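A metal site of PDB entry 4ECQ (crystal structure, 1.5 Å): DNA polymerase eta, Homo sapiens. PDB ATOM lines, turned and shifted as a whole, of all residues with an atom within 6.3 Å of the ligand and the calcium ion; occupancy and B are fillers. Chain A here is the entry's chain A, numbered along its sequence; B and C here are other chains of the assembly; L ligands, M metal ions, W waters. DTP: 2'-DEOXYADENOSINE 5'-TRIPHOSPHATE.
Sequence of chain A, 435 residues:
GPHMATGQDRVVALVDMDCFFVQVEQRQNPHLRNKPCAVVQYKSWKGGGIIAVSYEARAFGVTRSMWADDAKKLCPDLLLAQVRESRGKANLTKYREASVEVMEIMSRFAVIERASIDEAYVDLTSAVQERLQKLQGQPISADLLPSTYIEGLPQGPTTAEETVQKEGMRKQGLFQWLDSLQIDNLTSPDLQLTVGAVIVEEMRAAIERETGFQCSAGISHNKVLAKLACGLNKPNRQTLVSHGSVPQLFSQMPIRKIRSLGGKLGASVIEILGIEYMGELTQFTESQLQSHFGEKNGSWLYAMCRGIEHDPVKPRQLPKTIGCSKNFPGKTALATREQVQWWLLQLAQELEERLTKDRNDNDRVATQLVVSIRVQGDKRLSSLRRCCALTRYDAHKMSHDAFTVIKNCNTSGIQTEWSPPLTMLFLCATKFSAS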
ATOM      1  N   ASP A  16     -16.399  14.311 -12.216  1.00  0.00           N
ATOM      2  CA  ASP A  16     -15.161  13.941 -12.927  1.00  0.00           C
ATOM      3  C   ASP A  16     -15.066  14.876 -14.132  1.00  0.00           C
ATOM      4  O   ASP A  16     -15.913  14.805 -15.034  1.00  0.00           O
ATOM      5  CB  ASP A  16     -15.338  12.486 -13.373  1.00  0.00           C
ATOM      6  CG  ASP A  16     -14.075  11.848 -13.904  1.00  0.00           C
ATOM      7  OD1 ASP A  16     -14.061  10.599 -14.044  1.00  0.00           O
ATOM      8  OD2 ASP A  16     -13.119  12.560 -14.196  1.00  0.00           O
ATOM      9  N   MET A  17     -14.062  15.754 -14.175  1.00  0.00           N
ATOM     10  CA  MET A  17     -13.935  16.703 -15.285  1.00  0.00           C
ATOM     11  C   MET A  17     -13.693  15.957 -16.593  1.00  0.00           C
ATOM     12  O   MET A  17     -12.989  14.949 -16.627  1.00  0.00           O
ATOM     13  CB  MET A  17     -12.797  17.683 -15.033  1.00  0.00           C
ATOM     14  CG  MET A  17     -12.865  18.372 -13.664  1.00  0.00           C
ATOM     15  SD  MET A  17     -14.410  19.268 -13.404  1.00  0.00           S
ATOM     16  CE  MET A  17     -14.316  20.453 -14.712  1.00  0.00           C
ATOM     17  N   ASP A  18     -14.298  16.430 -17.669  1.00  0.00           N
ATOM     18  CA  ASP A  18     -14.066  15.783 -18.962  1.00  0.00           C
ATOM     19  C   ASP A  18     -12.689  16.173 -19.496  1.00  0.00           C
ATOM     20  O   ASP A  18     -12.269  17.354 -19.396  1.00  0.00           O
ATOM     21  CB  ASP A  18     -15.134  16.202 -19.954  1.00  0.00           C
ATOM     22  CG  ASP A  18     -16.541  15.769 -19.521  1.00  0.00           C
ATOM     23  OD1 ASP A  18     -16.657  14.707 -18.895  1.00  0.00           O
ATOM     24  OD2 ASP A  18     -17.505  16.476 -19.842  1.00  0.00           O
ATOM     25  N   CYS A  19     -11.998  15.178 -20.050  1.00  0.00           N
ATOM     26  CA  CYS A  19     -10.661  15.386 -20.656  1.00  0.00           C
ATOM     27  C   CYS A  19      -9.935  16.583 -20.058  1.00  0.00           C
ATOM     28  O   CYS A  19      -9.627  17.548 -20.749  1.00  0.00           O
ATOM     29  CB  CYS A  19     -10.743  15.474 -22.183  1.00  0.00           C
ATOM     30  SG  CYS A  19     -11.857  16.685 -22.912  1.00  0.00           S
ATOM     31  N   PHE A  20      -9.638  16.507 -18.758  1.00  0.00           N
ATOM     32  CA  PHE A  20      -9.366  17.719 -17.988  1.00  0.00           C
ATOM     33  C   PHE A  20      -8.199  18.558 -18.502  1.00  0.00           C
ATOM     34  O   PHE A  20      -8.361  19.765 -18.712  1.00  0.00           O
ATOM     35  CB  PHE A  20      -9.160  17.378 -16.508  1.00  0.00           C
ATOM     36  CG  PHE A  20      -8.971  18.588 -15.633  1.00  0.00           C
ATOM     37  CD1 PHE A  20      -9.872  19.641 -15.677  1.00  0.00           C
ATOM     38  CD2 PHE A  20      -7.916  18.637 -14.736  1.00  0.00           C
ATOM     39  CE1 PHE A  20      -9.694  20.763 -14.856  1.00  0.00           C
ATOM     40  CE2 PHE A  20      -7.747  19.768 -13.908  1.00  0.00           C
ATOM     41  CZ  PHE A  20      -8.639  20.803 -13.976  1.00  0.00           C
ATOM     42  N   PHE A  21      -7.008  17.974 -18.685  1.00  0.00           N
ATOM     43  CA  PHE A  21      -5.884  18.810 -19.082  1.00  0.00           C
ATOM     44  C   PHE A  21      -6.141  19.455 -20.453  1.00  0.00           C
ATOM     45  O   PHE A  21      -5.656  20.557 -20.709  1.00  0.00           O
ATOM     46  CB  PHE A  21      -4.546  18.048 -19.114  1.00  0.00           C
ATOM     47  CG  PHE A  21      -4.003  17.653 -17.771  1.00  0.00           C
ATOM     48  CD1 PHE A  21      -4.786  17.667 -16.625  1.00  0.00           C
ATOM     49  CD2 PHE A  21      -2.693  17.248 -17.667  1.00  0.00           C
ATOM     50  CE1 PHE A  21      -4.247  17.296 -15.397  1.00  0.00           C
ATOM     51  CE2 PHE A  21      -2.148  16.860 -16.442  1.00  0.00           C
ATOM     52  CZ  PHE A  21      -2.933  16.889 -15.315  1.00  0.00           C
ATOM     53  N   VAL A  22      -6.854  18.739 -21.325  1.00  0.00           N
ATOM     54  CA  VAL A  22      -7.244  19.289 -22.619  1.00  0.00           C
ATOM     55  C   VAL A  22      -8.121  20.517 -22.439  1.00  0.00           C
ATOM     56  O   VAL A  22      -7.883  21.550 -23.086  1.00  0.00           O
ATOM     57  CB  VAL A  22      -7.928  18.231 -23.488  1.00  0.00           C
ATOM     58  CG1 VAL A  22      -8.690  18.881 -24.658  1.00  0.00           C
ATOM     59  CG2 VAL A  22      -6.902  17.232 -24.000  1.00  0.00           C
ATOM     60  N   GLN A  41       3.632  15.404 -22.992  1.00  0.00           N
ATOM     61  CA  GLN A  41       4.758  15.883 -22.193  1.00  0.00           C
ATOM     62  C   GLN A  41       6.048  15.538 -22.906  1.00  0.00           C
ATOM     63  O   GLN A  41       6.198  14.445 -23.453  1.00  0.00           O
ATOM     64  CB  GLN A  41       4.728  15.336 -20.766  1.00  0.00           C
ATOM     65  CG  GLN A  41       4.469  13.859 -20.652  1.00  0.00           C
ATOM     66  CD  GLN A  41       4.131  13.467 -19.237  1.00  0.00           C
ATOM     67  OE1 GLN A  41       3.918  14.321 -18.376  1.00  0.00           O
ATOM     68  NE2 GLN A  41       4.091  12.165 -18.983  1.00  0.00           N
ATOM     69  N   ILE A  51      -0.915  12.486 -22.556  1.00  0.00           N
ATOM     70  CA  ILE A  51      -1.519  12.263 -21.251  1.00  0.00           C
ATOM     71  C   ILE A  51      -3.001  12.636 -21.174  1.00  0.00           C
ATOM     72  O   ILE A  51      -3.678  12.288 -20.198  1.00  0.00           O
ATOM     73  CB  ILE A  51      -0.736  12.967 -20.123  1.00  0.00           C
ATOM     74  CG1 ILE A  51      -0.669  14.487 -20.337  1.00  0.00           C
ATOM     75  CG2 ILE A  51       0.672  12.352 -20.009  1.00  0.00           C
ATOM     76  CD1 ILE A  51      -0.116  15.230 -19.101  1.00  0.00           C
ATOM     77  N   ALA A  52      -3.532  13.320 -22.185  1.00  0.00           N
ATOM     78  CA  ALA A  52      -4.971  13.643 -22.208  1.00  0.00           C
ATOM     79  C   ALA A  52      -5.408  13.867 -23.643  1.00  0.00           C
ATOM     80  O   ALA A  52      -4.639  14.369 -24.466  1.00  0.00           O
ATOM     81  CB  ALA A  52      -5.262  14.884 -21.353  1.00  0.00           C
ATOM     82  N   VAL A  53      -6.663  13.510 -23.948  1.00  0.00           N
ATOM     83  CA  VAL A  53      -7.162  13.463 -25.325  1.00  0.00           C
ATOM     84  C   VAL A  53      -8.593  13.981 -25.431  1.00  0.00           C
ATOM     85  O   VAL A  53      -9.470  13.536 -24.682  1.00  0.00           O
ATOM     86  CB  VAL A  53      -7.162  11.991 -25.833  1.00  0.00           C
ATOM     87  CG1 VAL A  53      -7.480  11.945 -27.328  1.00  0.00           C
ATOM     88  CG2 VAL A  53      -5.828  11.328 -25.578  1.00  0.00           C
ATOM     89  N   TYR A  55     -12.392  14.520 -26.904  1.00  0.00           N
ATOM     90  CA  TYR A  55     -13.324  13.511 -27.418  1.00  0.00           C
ATOM     91  C   TYR A  55     -13.314  13.433 -28.948  1.00  0.00           C
ATOM     92  O   TYR A  55     -13.482  12.367 -29.525  1.00  0.00           O
ATOM     93  CB  TYR A  55     -14.736  13.703 -26.812  1.00  0.00           C
ATOM     94  CG  TYR A  55     -14.799  13.182 -25.388  1.00  0.00           C
ATOM     95  CD1 TYR A  55     -14.264  13.910 -24.327  1.00  0.00           C
ATOM     96  CD2 TYR A  55     -15.293  11.912 -25.109  1.00  0.00           C
ATOM     97  CE1 TYR A  55     -14.260  13.421 -23.035  1.00  0.00           C
ATOM     98  CE2 TYR A  55     -15.312  11.417 -23.826  1.00  0.00           C
ATOM     99  CZ  TYR A  55     -14.789  12.158 -22.793  1.00  0.00           C
ATOM    100  OH  TYR A  55     -14.819  11.628 -21.513  1.00  0.00           O
ATOM    101  N   ARG A  58     -10.420  11.207 -29.659  1.00  0.00           N
ATOM    102  CA  ARG A  58     -10.693   9.804 -29.312  1.00  0.00           C
ATOM    103  C   ARG A  58     -11.434   9.072 -30.436  1.00  0.00           C
ATOM    104  O   ARG A  58     -11.240   7.853 -30.619  1.00  0.00           O
ATOM    105  CB  ARG A  58     -11.500   9.700 -28.021  1.00  0.00           C
ATOM    106  CG  ARG A  58     -10.786  10.296 -26.833  1.00  0.00           C
ATOM    107  CD  ARG A  58     -11.626  10.204 -25.571  1.00  0.00           C
ATOM    108  NE  ARG A  58     -11.078  11.098 -24.554  1.00  0.00           N
ATOM    109  CZ  ARG A  58     -11.351  11.019 -23.253  1.00  0.00           C
ATOM    110  NH1 ARG A  58     -12.184  10.095 -22.802  1.00  0.00           N
ATOM    111  NH2 ARG A  58     -10.787  11.906 -22.414  1.00  0.00           N
ATOM    112  N   ARG A  64      -4.425   7.958 -24.328  1.00  0.00           N
ATOM    113  CA  ARG A  64      -3.343   8.169 -23.382  1.00  0.00           C
ATOM    114  C   ARG A  64      -2.268   7.090 -23.533  1.00  0.00           C
ATOM    115  O   ARG A  64      -2.562   5.952 -23.898  1.00  0.00           O
ATOM    116  CB  ARG A  64      -3.920   8.171 -21.960  1.00  0.00           C
ATOM    117  CG  ARG A  64      -2.900   8.207 -20.826  1.00  0.00           C
ATOM    118  CD  ARG A  64      -3.621   8.401 -19.483  1.00  0.00           C
ATOM    119  NE  ARG A  64      -4.388   9.640 -19.482  1.00  0.00           N
ATOM    120  CZ  ARG A  64      -5.663   9.748 -19.095  1.00  0.00           C
ATOM    121  NH1 ARG A  64      -6.319   8.675 -18.658  1.00  0.00           N
ATOM    122  NH2 ARG A  64      -6.271  10.930 -19.135  1.00  0.00           N
ATOM    123  N   SER A 116      -8.775  12.971  -6.840  1.00  0.00           N
ATOM    124  CA  SER A 116      -7.667  13.100  -7.774  1.00  0.00           C
ATOM    125  C   SER A 116      -7.624  14.546  -8.255  1.00  0.00           C
ATOM    126  O   SER A 116      -8.420  15.368  -7.810  1.00  0.00           O
ATOM    127  CB  SER A 116      -7.880  12.204  -8.990  1.00  0.00           C
ATOM    128  OG  SER A 116      -8.902  12.731  -9.838  1.00  0.00           O
ATOM    129  N   ILE A 117      -6.725  14.844  -9.186  1.00  0.00           N
ATOM    130  CA  ILE A 117      -6.611  16.202  -9.700  1.00  0.00           C
ATOM    131  C   ILE A 117      -7.936  16.716 -10.307  1.00  0.00           C
ATOM    132  O   ILE A 117      -8.199  17.913 -10.327  1.00  0.00           O
ATOM    133  CB  ILE A 117      -5.461  16.316 -10.718  1.00  0.00           C
ATOM    134  CG1 ILE A 117      -5.056  17.788 -10.878  1.00  0.00           C
ATOM    135  CG2 ILE A 117      -5.813  15.647 -12.032  1.00  0.00           C
ATOM    136  CD1 ILE A 117      -3.653  17.988 -11.447  1.00  0.00           C
ATOM    137  N   ASP A 118      -8.784  15.805 -10.797  1.00  0.00           N
ATOM    138  CA  ASP A 118     -10.014  16.261 -11.454  1.00  0.00           C
ATOM    139  C   ASP A 118     -11.282  15.541 -11.049  1.00  0.00           C
ATOM    140  O   ASP A 118     -12.298  15.599 -11.767  1.00  0.00           O
ATOM    141  CB  ASP A 118      -9.840  16.230 -12.966  1.00  0.00           C
ATOM    142  CG  ASP A 118     -10.099  14.873 -13.544  1.00  0.00           C
ATOM    143  OD1 ASP A 118     -10.637  14.813 -14.662  1.00  0.00           O
ATOM    144  OD2 ASP A 118      -9.792  13.852 -12.857  1.00  0.00           O
ATOM    145  N   GLU A 119     -11.255  14.867  -9.897  1.00  0.00           N
ATOM    146  CA  GLU A 119     -12.413  14.138  -9.398  1.00  0.00           C
ATOM    147  C   GLU A 119     -12.638  14.452  -7.947  1.00  0.00           C
ATOM    148  O   GLU A 119     -11.682  14.535  -7.157  1.00  0.00           O
ATOM    149  CB  GLU A 119     -12.188  12.625  -9.490  1.00  0.00           C
ATOM    150  CG  GLU A 119     -12.057  12.089 -10.908  1.00  0.00           C
ATOM    151  CD  GLU A 119     -12.073  10.581 -10.964  1.00  0.00           C
ATOM    152  OE1 GLU A 119     -12.408   9.947  -9.940  1.00  0.00           O
ATOM    153  OE2 GLU A 119     -11.754  10.015 -12.040  1.00  0.00           O
ATOM    154  N   LYS A 234     -20.584   9.785 -20.672  1.00  0.00           N
ATOM    155  CA  LYS A 234     -19.586  10.846 -20.745  1.00  0.00           C
ATOM    156  C   LYS A 234     -19.519  11.204 -22.216  1.00  0.00           C
ATOM    157  O   LYS A 234     -19.783  10.367 -23.077  1.00  0.00           O
ATOM    158  CB  LYS A 234     -18.224  10.331 -20.286  1.00  0.00           C
ATOM    159  CG  LYS A 234     -17.872  10.617 -18.820  1.00  0.00           C
ATOM    160  CD  LYS A 234     -16.329  10.766 -18.680  1.00  0.00           C
ATOM    161  CE  LYS A 234     -15.889  11.318 -17.304  1.00  0.00           C
ATOM    162  NZ  LYS A 234     -15.420  12.760 -17.335  1.00  0.00           N
ATOM    163  N   PRO A 235     -19.187  12.459 -22.519  1.00  0.00           N
ATOM    164  CA  PRO A 235     -18.878  13.546 -21.591  1.00  0.00           C
ATOM    165  C   PRO A 235     -20.093  14.442 -21.372  1.00  0.00           C
ATOM    166  O   PRO A 235     -21.127  14.293 -22.034  1.00  0.00           O
ATOM    167  CB  PRO A 235     -17.844  14.334 -22.370  1.00  0.00           C
ATOM    168  CG  PRO A 235     -18.349  14.245 -23.803  1.00  0.00           C
ATOM    169  CD  PRO A 235     -18.947  12.852 -23.922  1.00  0.00           C
ATOM    170  P    DT B   3       7.671   2.161 -23.467  1.00  0.00           P
ATOM    171  OP1  DT B   3       8.327   0.833 -23.497  1.00  0.00           O
ATOM    172  OP2  DT B   3       6.628   2.499 -24.451  1.00  0.00           O
ATOM    173  O5'  DT B   3       7.060   2.360 -22.003  1.00  0.00           O
ATOM    174  C5'  DT B   3       6.008   3.294 -21.785  1.00  0.00           C
ATOM    175  C4'  DT B   3       6.539   4.715 -21.715  1.00  0.00           C
ATOM    176  O4'  DT B   3       5.430   5.641 -21.868  1.00  0.00           O
ATOM    177  C3'  DT B   3       7.212   5.103 -20.402  1.00  0.00           C
ATOM    178  O3'  DT B   3       8.204   6.088 -20.661  1.00  0.00           O
ATOM    179  C2'  DT B   3       6.050   5.675 -19.598  1.00  0.00           C
ATOM    180  C1'  DT B   3       5.269   6.403 -20.685  1.00  0.00           C
ATOM    181  N1   DT B   3       3.800   6.508 -20.418  1.00  0.00           N
ATOM    182  C2   DT B   3       3.172   7.730 -20.513  1.00  0.00           C
ATOM    183  O2   DT B   3       3.739   8.764 -20.825  1.00  0.00           O
ATOM    184  N3   DT B   3       1.828   7.705 -20.246  1.00  0.00           N
ATOM    185  C4   DT B   3       1.070   6.606 -19.895  1.00  0.00           C
ATOM    186  O4   DT B   3      -0.135   6.678 -19.672  1.00  0.00           O
ATOM    187  C5   DT B   3       1.785   5.353 -19.807  1.00  0.00           C
ATOM    188  C7   DT B   3       1.081   4.083 -19.433  1.00  0.00           C
ATOM    189  C6   DT B   3       3.103   5.369 -20.069  1.00  0.00           C
ATOM    190  P    DT B   4       8.968   6.808 -19.451  1.00  0.00           P
ATOM    191  OP1  DT B   4      10.142   7.521 -20.010  1.00  0.00           O
ATOM    192  OP2  DT B   4       9.138   5.840 -18.358  1.00  0.00           O
ATOM    193  O5'  DT B   4       7.904   7.906 -18.947  1.00  0.00           O
ATOM    194  C5'  DT B   4       7.752   9.095 -19.693  1.00  0.00           C
ATOM    195  C4'  DT B   4       7.178  10.143 -18.772  1.00  0.00           C
ATOM    196  O4'  DT B   4       5.776   9.844 -18.537  1.00  0.00           O
ATOM    197  C3'  DT B   4       7.794  10.253 -17.387  1.00  0.00           C
ATOM    198  O3'  DT B   4       7.824  11.636 -17.104  1.00  0.00           O
ATOM    199  C2'  DT B   4       6.809   9.511 -16.485  1.00  0.00           C
ATOM    200  C1'  DT B   4       5.499   9.891 -17.145  1.00  0.00           C
ATOM    201  N1   DT B   4       4.374   8.948 -16.963  1.00  0.00           N
ATOM    202  C2   DT B   4       3.130   9.521 -16.864  1.00  0.00           C
ATOM    203  O2   DT B   4       2.970  10.725 -16.902  1.00  0.00           O
ATOM    204  N3   DT B   4       2.107   8.637 -16.716  1.00  0.00           N
ATOM    205  C4   DT B   4       2.186   7.262 -16.675  1.00  0.00           C
ATOM    206  O4   DT B   4       1.188   6.568 -16.540  1.00  0.00           O
ATOM    207  C5   DT B   4       3.530   6.725 -16.784  1.00  0.00           C
ATOM    208  C7   DT B   4       3.752   5.238 -16.742  1.00  0.00           C
ATOM    209  C6   DT B   4       4.546   7.588 -16.932  1.00  0.00           C
ATOM    210  P    DA B   5       8.422  12.180 -15.726  1.00  0.00           P
ATOM    211  OP1  DA B   5       9.244  13.366 -16.023  1.00  0.00           O
ATOM    212  OP2  DA B   5       9.045  11.033 -15.011  1.00  0.00           O
ATOM    213  O5'  DA B   5       7.138  12.600 -14.894  1.00  0.00           O
ATOM    214  C5'  DA B   5       6.376  13.742 -15.307  1.00  0.00           C
ATOM    215  C4'  DA B   5       5.248  13.976 -14.331  1.00  0.00           C
ATOM    216  O4'  DA B   5       4.289  12.881 -14.423  1.00  0.00           O
ATOM    217  C3'  DA B   5       5.695  14.010 -12.866  1.00  0.00           C
ATOM    218  O3'  DA B   5       4.938  15.020 -12.206  1.00  0.00           O
ATOM    219  C2'  DA B   5       5.313  12.618 -12.363  1.00  0.00           C
ATOM    220  C1'  DA B   5       4.002  12.433 -13.114  1.00  0.00           C
ATOM    221  N9   DA B   5       3.578  11.040 -13.179  1.00  0.00           N
ATOM    222  C8   DA B   5       4.373   9.937 -13.311  1.00  0.00           C
ATOM    223  N7   DA B   5       3.693   8.802 -13.363  1.00  0.00           N
ATOM    224  C5   DA B   5       2.373   9.188 -13.263  1.00  0.00           C
ATOM    225  C6   DA B   5       1.168   8.457 -13.252  1.00  0.00           C
ATOM    226  N6   DA B   5       1.102   7.123 -13.344  1.00  0.00           N
ATOM    227  N1   DA B   5       0.027   9.169 -13.151  1.00  0.00           N
ATOM    228  C2   DA B   5       0.081  10.503 -13.047  1.00  0.00           C
ATOM    229  N3   DA B   5       1.155  11.300 -13.046  1.00  0.00           N
ATOM    230  C4   DA B   5       2.267  10.560 -13.154  1.00  0.00           C
ATOM    231  P    DT C   8      -9.773   6.122 -10.847  1.00  0.00           P
ATOM    232  OP1  DT C   8     -10.101   6.106  -9.409  1.00  0.00           O
ATOM    233  OP2  DT C   8     -10.825   6.363 -11.857  1.00  0.00           O
ATOM    234  O5'  DT C   8      -8.652   7.207 -11.152  1.00  0.00           O
ATOM    235  C5'  DT C   8      -9.058   8.343 -11.842  1.00  0.00           C
ATOM    236  C4'  DT C   8      -8.188   9.520 -11.497  1.00  0.00           C
ATOM    237  O4'  DT C   8      -6.820   9.082 -11.229  1.00  0.00           O
ATOM    238  C3'  DT C   8      -8.130  10.525 -12.649  1.00  0.00           C
ATOM    239  O3'  DT C   8      -8.173  11.841 -12.146  1.00  0.00           O
ATOM    240  C2'  DT C   8      -6.772  10.223 -13.297  1.00  0.00           C
ATOM    241  C1'  DT C   8      -5.937   9.766 -12.096  1.00  0.00           C
ATOM    242  N1   DT C   8      -4.853   8.814 -12.476  1.00  0.00           N
ATOM    243  C2   DT C   8      -3.573   9.286 -12.586  1.00  0.00           C
ATOM    244  O2   DT C   8      -3.271  10.466 -12.427  1.00  0.00           O
ATOM    245  N3   DT C   8      -2.635   8.334 -12.929  1.00  0.00           N
ATOM    246  C4   DT C   8      -2.843   6.991 -13.151  1.00  0.00           C
ATOM    247  O4   DT C   8      -1.938   6.217 -13.442  1.00  0.00           O
ATOM    248  C5   DT C   8      -4.210   6.565 -13.006  1.00  0.00           C
ATOM    249  C7   DT C   8      -4.544   5.111 -13.221  1.00  0.00           C
ATOM    250  C6   DT C   8      -5.137   7.480 -12.678  1.00  0.00           C
HETATM  251  PG  DTP L   1     -12.175  11.688 -19.160  1.00  0.00           P
HETATM  252  O1G DTP L   1     -12.204  10.269 -19.708  1.00  0.00           O
HETATM  253  O2G DTP L   1     -13.047  12.681 -19.866  1.00  0.00           O
HETATM  254  O3G DTP L   1     -12.284  11.748 -17.653  1.00  0.00           O
HETATM  255  PB  DTP L   1      -9.546  12.767 -18.568  1.00  0.00           P
HETATM  256  O1B DTP L   1     -10.143  13.748 -17.588  1.00  0.00           O
HETATM  257  O2B DTP L   1      -8.395  13.247 -19.410  1.00  0.00           O
HETATM  258  O3B DTP L   1     -10.661  12.163 -19.562  1.00  0.00           O
HETATM  259  PA  DTP L   1      -8.817  11.150 -16.245  1.00  0.00           P
HETATM  260  O1A DTP L   1      -8.336   9.710 -16.176  1.00  0.00           O
HETATM  261  O2A DTP L   1     -10.043  11.526 -15.469  1.00  0.00           O
HETATM  262  O3A DTP L   1      -9.017  11.455 -17.830  1.00  0.00           O
HETATM  263  O5' DTP L   1      -7.561  12.040 -15.797  1.00  0.00           O
HETATM  264  C5' DTP L   1      -7.657  13.420 -15.419  1.00  0.00           C
HETATM  265  C4' DTP L   1      -6.350  14.102 -15.815  1.00  0.00           C
HETATM  266  O4' DTP L   1      -5.255  13.495 -15.119  1.00  0.00           O
HETATM  267  C3' DTP L   1      -6.029  13.924 -17.296  1.00  0.00           C
HETATM  268  O3' DTP L   1      -6.604  14.944 -18.114  1.00  0.00           O
HETATM  269  C2' DTP L   1      -4.510  13.971 -17.294  1.00  0.00           C
HETATM  270  C1' DTP L   1      -4.108  13.355 -15.953  1.00  0.00           C
HETATM  271  N9  DTP L   1      -3.807  11.901 -16.055  1.00  0.00           N
HETATM  272  C8  DTP L   1      -4.675  10.889 -16.012  1.00  0.00           C
HETATM  273  N7  DTP L   1      -3.995   9.713 -16.125  1.00  0.00           N
HETATM  274  C5  DTP L   1      -2.685  10.023 -16.239  1.00  0.00           C
HETATM  275  C6  DTP L   1      -1.521   9.273 -16.366  1.00  0.00           C
HETATM  276  N6  DTP L   1      -1.570   7.914 -16.422  1.00  0.00           N
HETATM  277  N1  DTP L   1      -0.327   9.903 -16.458  1.00  0.00           N
HETATM  278  C2  DTP L   1      -0.263  11.242 -16.403  1.00  0.00           C
HETATM  279  N3  DTP L   1      -1.361  12.002 -16.272  1.00  0.00           N
HETATM  280  C4  DTP L   1      -2.575  11.402 -16.184  1.00  0.00           C
HETATM  281 CA    CA M   1     -11.705  13.189 -15.955  1.00  0.00          CA
HETATM  282  O   HOH W   1      -3.617  12.899 -12.811  1.00  0.00           O
HETATM  283  O   HOH W   2      -7.887  12.164 -21.825  1.00  0.00           O
HETATM  284  O   HOH W   3      -4.641   7.041 -16.332  1.00  0.00           O
HETATM  285  O   HOH W   4      -0.366  14.390 -15.120  1.00  0.00           O
HETATM  286  O   HOH W   5     -12.732   8.511 -17.545  1.00  0.00           O
HETATM  287  O   HOH W   6      -6.984   7.468 -15.323  1.00  0.00           O
HETATM  288  O   HOH W   7      -3.222   5.126 -17.628  1.00  0.00           O
HETATM  289  O   HOH W   8     -11.780   9.442 -14.870  1.00  0.00           O
HETATM  290  O   HOH W   9     -10.193   8.552 -20.235  1.00  0.00           O
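O of Met 17 is bound to the calcium ion (2.3 Å). An oxygen (O3G) of the ligand binds the calcium ion, at 2.3 Å. O1B of the ligand is bound to the calcium ion (2.3 Å). The calcium ion is bound by OD1 of Asp 118 (2.3 Å). The side-chain carboxylate (OD2) of Asp 16 is bound to the calcium ion (2.3 Å). O2A of the ligand binds the calcium ion, at 2.4 Å.
O of Met 17 sits close to NZ of Lys 234, at 3.3 Å. OD2 of Asp 118 sits close to O3' of DT 8 of chain C, 2.7 Å away. OG of Ser 116 sits close to N of Asp 118, at 3.2 Å. The side-chain amino group of Lys 234 is in hydrogen-bond range of the backbone carbonyl oxygen of Asp 16 (3.1 Å). OH of Tyr 55 sits at hydrogen-bond distance from NH1 of Arg 58. O2 of DT 4 of chain B is in hydrogen-bond range of the side-chain amide nitrogen (NE2) of Gln 41, 2.8 Å away. The backbone carbonyl oxygen of Ile 51 is in hydrogen-bond range of the guanidinium group of Arg 64 (2.8 Å). O3' of DT 8 of chain C lies within hydrogen-bond range of the side-chain hydroxyl of Ser 116 (2.6 Å).
Water W3 lies within hydrogen-bond range of N7 of the ligand (2.8 Å) and NH1 of Arg 64 (3.3 Å). Water W8 bridges OD1 of Asp 16 (2.7 Å) and OE2 of Glu 119 (2.9 Å). Water W1 bridges O2 of DT 8 of chain C (2.5 Å) and an oxygen (O4') of the ligand (2.9 Å).
Lys 234 touches the calcium ion.
O2G of the ligand sits at hydrogen-bond distance from OH of Tyr 55 (2.6 Å). The backbone NH of Cys 19 sits at hydrogen-bond distance from an oxygen (O2G) of the ligand (2.7 Å). A nitrogen (N6) of the ligand sits at hydrogen-bond distance from O4 of DT 4 of chain B (3.1 Å). The guanidinium group (NH1) of Arg 58 is in salt-bridge range of an oxygen (O1G) of the ligand (3.1 Å). The backbone NH (N) of Phe 20 sits at hydrogen-bond distance from an oxygen (O3') of the ligand, 3.5 Å away. NH2 of Arg 64 is in salt-bridge range of O2B of the ligand (3.2 Å). An oxygen (O3') of the ligand sits at hydrogen-bond distance from the backbone NH of Phe 21 (3.1 Å). O4 of DT 8 of chain C sits at hydrogen-bond distance from a nitrogen (N6) of the ligand. The side-chain amino group of Lys 234 lies within salt-bridge range of an oxygen (O2G) of the ligand, 3.5 Å away.
N1 of DA 5 of chain B lies close to a nitrogen (N1) of the ligand (3.4 Å). Residues that only touch the ligand: Asp 18, Ile 51, Ala 52, Ile 117 and DT 3 of chain B. Hydrophobic or aromatic side chains within 4 Å of the ligand: Phe 20, Phe 21, Ile 51, Ala 52, Tyr 55 and Ile 117. Of the 24 residues printed, 18 come within 4 Å of the ligand. The nearest printed residue that does not touch the ligand is Glu 119 (4.1 Å).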
